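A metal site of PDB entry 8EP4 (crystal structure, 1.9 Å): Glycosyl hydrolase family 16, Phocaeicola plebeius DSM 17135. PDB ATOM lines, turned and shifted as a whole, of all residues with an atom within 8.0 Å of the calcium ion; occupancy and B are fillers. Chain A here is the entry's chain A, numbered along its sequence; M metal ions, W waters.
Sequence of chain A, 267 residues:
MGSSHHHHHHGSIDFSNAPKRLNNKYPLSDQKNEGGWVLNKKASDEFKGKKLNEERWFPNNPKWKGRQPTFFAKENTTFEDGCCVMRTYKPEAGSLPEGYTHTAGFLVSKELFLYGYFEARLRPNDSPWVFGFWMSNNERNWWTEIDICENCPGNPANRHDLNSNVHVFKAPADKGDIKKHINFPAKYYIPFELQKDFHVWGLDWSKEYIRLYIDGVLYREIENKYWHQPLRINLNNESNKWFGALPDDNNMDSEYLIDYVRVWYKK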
ATOM      1  N   ASP A  45     -11.948  13.994 -14.747  1.00  0.00           N
ATOM      2  CA  ASP A  45     -11.882  15.453 -14.791  1.00  0.00           C
ATOM      3  C   ASP A  45     -11.781  16.003 -13.378  1.00  0.00           C
ATOM      4  O   ASP A  45     -12.682  15.791 -12.557  1.00  0.00           O
ATOM      5  CB  ASP A  45     -13.104  16.033 -15.512  1.00  0.00           C
ATOM      6  CG  ASP A  45     -12.829  17.383 -16.111  1.00  0.00           C
ATOM      7  OD1 ASP A  45     -12.033  18.144 -15.527  1.00  0.00           O
ATOM      8  OD2 ASP A  45     -13.396  17.679 -17.191  1.00  0.00           O
ATOM      9  N   GLU A  46     -10.700  16.711 -13.085  1.00  0.00           N
ATOM     10  CA  GLU A  46     -10.539  17.392 -11.800  1.00  0.00           C
ATOM     11  C   GLU A  46     -11.179  18.780 -11.800  1.00  0.00           C
ATOM     12  O   GLU A  46     -11.142  19.464 -10.771  1.00  0.00           O
ATOM     13  CB  GLU A  46      -9.049  17.500 -11.462  1.00  0.00           C
ATOM     14  CG  GLU A  46      -8.352  16.140 -11.310  1.00  0.00           C
ATOM     15  CD  GLU A  46      -8.981  15.254 -10.223  1.00  0.00           C
ATOM     16  OE1 GLU A  46      -9.088  15.721  -9.050  1.00  0.00           O
ATOM     17  OE2 GLU A  46      -9.387  14.106 -10.539  1.00  0.00           O
ATOM     18  N   PHE A  47     -11.675  19.242 -12.963  1.00  0.00           N
ATOM     19  CA  PHE A  47     -12.405  20.514 -13.088  1.00  0.00           C
ATOM     20  C   PHE A  47     -11.567  21.719 -12.633  1.00  0.00           C
ATOM     21  O   PHE A  47     -12.061  22.625 -11.969  1.00  0.00           O
ATOM     22  CB  PHE A  47     -13.747  20.434 -12.349  1.00  0.00           C
ATOM     23  CG  PHE A  47     -14.723  19.522 -13.026  1.00  0.00           C
ATOM     24  CD1 PHE A  47     -15.003  19.686 -14.378  1.00  0.00           C
ATOM     25  CD2 PHE A  47     -15.315  18.479 -12.344  1.00  0.00           C
ATOM     26  CE1 PHE A  47     -15.892  18.853 -15.026  1.00  0.00           C
ATOM     27  CE2 PHE A  47     -16.231  17.630 -12.991  1.00  0.00           C
ATOM     28  CZ  PHE A  47     -16.510  17.822 -14.334  1.00  0.00           C
ATOM     29  N   LYS A  48     -10.298  21.731 -13.005  1.00  0.00           N
ATOM     30  CA  LYS A  48      -9.486  22.914 -12.808  1.00  0.00           C
ATOM     31  C   LYS A  48      -9.693  23.908 -13.952  1.00  0.00           C
ATOM     32  O   LYS A  48     -10.273  23.590 -14.985  1.00  0.00           O
ATOM     33  CB  LYS A  48      -8.006  22.532 -12.714  1.00  0.00           C
ATOM     34  CG  LYS A  48      -7.702  21.484 -11.655  1.00  0.00           C
ATOM     35  CD  LYS A  48      -6.232  21.079 -11.747  1.00  0.00           C
ATOM     36  CE  LYS A  48      -6.017  19.679 -11.204  1.00  0.00           C
ATOM     37  NZ  LYS A  48      -6.128  19.628  -9.728  1.00  0.00           N
ATOM     38  N   GLY A  49      -9.240  25.140 -13.732  1.00  0.00           N
ATOM     39  CA  GLY A  49      -9.328  26.143 -14.786  1.00  0.00           C
ATOM     40  C   GLY A  49     -10.635  26.907 -14.756  1.00  0.00           C
ATOM     41  O   GLY A  49     -11.389  26.873 -13.771  1.00  0.00           O
ATOM     42  N   GLU A  80     -14.965  27.241 -11.295  1.00  0.00           N
ATOM     43  CA  GLU A  80     -14.482  28.170 -10.290  1.00  0.00           C
ATOM     44  C   GLU A  80     -13.789  27.394  -9.182  1.00  0.00           C
ATOM     45  O   GLU A  80     -14.345  26.428  -8.666  1.00  0.00           O
ATOM     46  CB  GLU A  80     -15.662  28.993  -9.725  1.00  0.00           C
ATOM     47  CG  GLU A  80     -16.555  29.553 -10.830  1.00  0.00           C
ATOM     48  CD  GLU A  80     -17.922  30.068 -10.370  1.00  0.00           C
ATOM     49  OE1 GLU A  80     -18.218  30.116  -9.151  1.00  0.00           O
ATOM     50  OE2 GLU A  80     -18.709  30.419 -11.273  1.00  0.00           O
ATOM     51  N   ASP A  81     -12.548  27.780  -8.862  1.00  0.00           N
ATOM     52  CA  ASP A  81     -11.864  27.279  -7.662  1.00  0.00           C
ATOM     53  C   ASP A  81     -11.791  25.760  -7.622  1.00  0.00           C
ATOM     54  O   ASP A  81     -11.985  25.143  -6.576  1.00  0.00           O
ATOM     55  CB  ASP A  81     -12.514  27.792  -6.379  1.00  0.00           C
ATOM     56  CG  ASP A  81     -11.647  27.532  -5.148  1.00  0.00           C
ATOM     57  OD1 ASP A  81     -10.459  27.944  -5.154  1.00  0.00           O
ATOM     58  OD2 ASP A  81     -12.128  26.898  -4.184  1.00  0.00           O
ATOM     59  N   GLY A  82     -11.536  25.139  -8.765  1.00  0.00           N
ATOM     60  CA  GLY A  82     -11.393  23.707  -8.822  1.00  0.00           C
ATOM     61  C   GLY A  82     -12.680  22.930  -8.890  1.00  0.00           C
ATOM     62  O   GLY A  82     -12.646  21.692  -8.759  1.00  0.00           O
ATOM     63  N   CYS A  83     -13.811  23.588  -9.136  1.00  0.00           N
ATOM     64  CA  CYS A  83     -15.114  22.928  -9.231  1.00  0.00           C
ATOM     65  C   CYS A  83     -15.862  23.317 -10.490  1.00  0.00           C
ATOM     66  O   CYS A  83     -15.789  24.460 -10.948  1.00  0.00           O
ATOM     67  CB  CYS A  83     -16.021  23.282  -8.028  1.00  0.00           C
ATOM     68  SG  CYS A  83     -15.491  22.562  -6.493  1.00  0.00           S
ATOM     69  N   CYS A  84     -16.582  22.356 -11.037  1.00  0.00           N
ATOM     70  CA  CYS A  84     -17.704  22.666 -11.900  1.00  0.00           C
ATOM     71  C   CYS A  84     -18.868  23.174 -11.020  1.00  0.00           C
ATOM     72  O   CYS A  84     -19.153  22.601  -9.961  1.00  0.00           O
ATOM     73  CB  CYS A  84     -18.099  21.429 -12.702  1.00  0.00           C
ATOM     74  SG  CYS A  84     -19.560  21.622 -13.725  1.00  0.00           S
ATOM     75  N   ARG A 121     -17.113  13.715  -6.418  1.00  0.00           N
ATOM     76  CA  ARG A 121     -17.172  14.433  -5.149  1.00  0.00           C
ATOM     77  C   ARG A 121     -18.056  15.652  -5.354  1.00  0.00           C
ATOM     78  O   ARG A 121     -17.756  16.498  -6.193  1.00  0.00           O
ATOM     79  CB  ARG A 121     -15.769  14.809  -4.664  1.00  0.00           C
ATOM     80  CG  ARG A 121     -15.758  15.532  -3.302  1.00  0.00           C
ATOM     81  CD  ARG A 121     -14.338  15.569  -2.716  1.00  0.00           C
ATOM     82  NE  ARG A 121     -14.353  16.130  -1.373  1.00  0.00           N
ATOM     83  CZ  ARG A 121     -14.096  17.403  -1.096  1.00  0.00           C
ATOM     84  NH1 ARG A 121     -13.741  18.260  -2.043  1.00  0.00           N
ATOM     85  NH2 ARG A 121     -14.227  17.833   0.157  1.00  0.00           N
ATOM     86  N   PHE A 198     -19.326  18.589   1.004  1.00  0.00           N
ATOM     87  CA  PHE A 198     -18.988  17.653  -0.056  1.00  0.00           C
ATOM     88  C   PHE A 198     -19.133  16.214   0.442  1.00  0.00           C
ATOM     89  O   PHE A 198     -18.805  15.910   1.587  1.00  0.00           O
ATOM     90  CB  PHE A 198     -17.537  17.862  -0.523  1.00  0.00           C
ATOM     91  CG  PHE A 198     -17.362  19.008  -1.481  1.00  0.00           C
ATOM     92  CD1 PHE A 198     -17.555  18.826  -2.844  1.00  0.00           C
ATOM     93  CD2 PHE A 198     -17.040  20.266  -1.014  1.00  0.00           C
ATOM     94  CE1 PHE A 198     -17.418  19.873  -3.734  1.00  0.00           C
ATOM     95  CE2 PHE A 198     -16.890  21.331  -1.910  1.00  0.00           C
ATOM     96  CZ  PHE A 198     -17.078  21.120  -3.258  1.00  0.00           C
ATOM     97  N   ILE A 258     -19.249  20.311  -8.297  1.00  0.00           N
ATOM     98  CA  ILE A 258     -18.638  19.024  -8.631  1.00  0.00           C
ATOM     99  C   ILE A 258     -17.142  19.233  -8.581  1.00  0.00           C
ATOM    100  O   ILE A 258     -16.569  19.925  -9.447  1.00  0.00           O
ATOM    101  CB  ILE A 258     -19.092  18.485  -9.994  1.00  0.00           C
ATOM    102  CG1 ILE A 258     -20.619  18.396 -10.035  1.00  0.00           C
ATOM    103  CG2 ILE A 258     -18.463  17.087 -10.322  1.00  0.00           C
ATOM    104  CD1 ILE A 258     -21.263  19.360 -11.019  1.00  0.00           C
ATOM    105  N   ASP A 259     -16.498  18.701  -7.537  1.00  0.00           N
ATOM    106  CA  ASP A 259     -15.057  18.835  -7.384  1.00  0.00           C
ATOM    107  C   ASP A 259     -14.322  17.989  -8.431  1.00  0.00           C
ATOM    108  O   ASP A 259     -13.351  18.458  -9.039  1.00  0.00           O
ATOM    109  CB  ASP A 259     -14.678  18.426  -5.959  1.00  0.00           C
ATOM    110  CG  ASP A 259     -13.208  18.643  -5.661  1.00  0.00           C
ATOM    111  OD1 ASP A 259     -12.535  19.377  -6.414  1.00  0.00           O
ATOM    112  OD2 ASP A 259     -12.729  18.060  -4.668  1.00  0.00           O
ATOM    113  N   TYR A 260     -14.763  16.762  -8.657  1.00  0.00           N
ATOM    114  CA  TYR A 260     -14.146  15.923  -9.677  1.00  0.00           C
ATOM    115  C   TYR A 260     -15.099  14.803 -10.067  1.00  0.00           C
ATOM    116  O   TYR A 260     -16.045  14.475  -9.352  1.00  0.00           O
ATOM    117  CB  TYR A 260     -12.829  15.316  -9.175  1.00  0.00           C
ATOM    118  CG  TYR A 260     -12.964  14.324  -8.029  1.00  0.00           C
ATOM    119  CD1 TYR A 260     -13.502  13.057  -8.226  1.00  0.00           C
ATOM    120  CD2 TYR A 260     -12.488  14.649  -6.747  1.00  0.00           C
ATOM    121  CE1 TYR A 260     -13.588  12.155  -7.198  1.00  0.00           C
ATOM    122  CE2 TYR A 260     -12.578  13.748  -5.710  1.00  0.00           C
ATOM    123  CZ  TYR A 260     -13.129  12.512  -5.937  1.00  0.00           C
ATOM    124  OH  TYR A 260     -13.199  11.607  -4.913  1.00  0.00           O
ATOM    125  N   VAL A 261     -14.804  14.218 -11.218  1.00  0.00           N
ATOM    126  CA  VAL A 261     -15.314  12.907 -11.627  1.00  0.00           C
ATOM    127  C   VAL A 261     -14.102  12.055 -11.948  1.00  0.00           C
ATOM    128  O   VAL A 261     -13.228  12.481 -12.712  1.00  0.00           O
ATOM    129  CB  VAL A 261     -16.234  13.033 -12.858  1.00  0.00           C
ATOM    130  CG1 VAL A 261     -16.584  11.663 -13.414  1.00  0.00           C
ATOM    131  CG2 VAL A 261     -17.515  13.811 -12.515  1.00  0.00           C
ATOM    132  N   ARG A 262     -14.021  10.859 -11.358  1.00  0.00           N
ATOM    133  CA  ARG A 262     -12.917   9.940 -11.631  1.00  0.00           C
ATOM    134  C   ARG A 262     -13.458   8.590 -12.093  1.00  0.00           C
ATOM    135  O   ARG A 262     -14.464   8.105 -11.573  1.00  0.00           O
ATOM    136  CB  ARG A 262     -12.036   9.728 -10.398  1.00  0.00           C
ATOM    137  CG  ARG A 262     -11.133  10.919 -10.100  1.00  0.00           C
ATOM    138  CD  ARG A 262     -10.503  10.839  -8.699  1.00  0.00           C
ATOM    139  NE  ARG A 262      -9.932  12.131  -8.350  1.00  0.00           N
ATOM    140  CZ  ARG A 262      -9.563  12.503  -7.126  1.00  0.00           C
ATOM    141  NH1 ARG A 262      -9.718  11.699  -6.081  1.00  0.00           N
ATOM    142  NH2 ARG A 262      -9.014  13.703  -6.962  1.00  0.00           N
HETATM  143 CA    CA M   1     -11.465  19.749  -8.512  1.00  0.00          CA
HETATM  144  O   HOH W   1     -10.249  17.877  -7.878  1.00  0.00           O
HETATM  145  O   HOH W   2      -9.331  20.889  -7.989  1.00  0.00           O
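The side-chain carboxylate (OE1) of Glu 46 lies within salt-bridge range of the guanidinium group (NH2) of Arg 262, at 2.9 Å. NH1 of Arg 121 is in salt-bridge range of OD2 of Asp 259 (2.8 Å).
The nearest printed residue that does not touch the calcium ion is Tyr 260 (4.5 Å).
The calcium ion is bound by O of Gly 82 (2.3 Å). The calcium ion is bound by O of Glu 46, at 2.3 Å. The calcium ion is bound by water W1 (2.3 Å). O of Asp 259 is bound to the calcium ion, at 2.3 Å. OD1 of Asp 259 is bound to the calcium ion (2.4 Å). Water W2 is bound to the calcium ion. The calcium ion has six donor atoms within binding distance.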
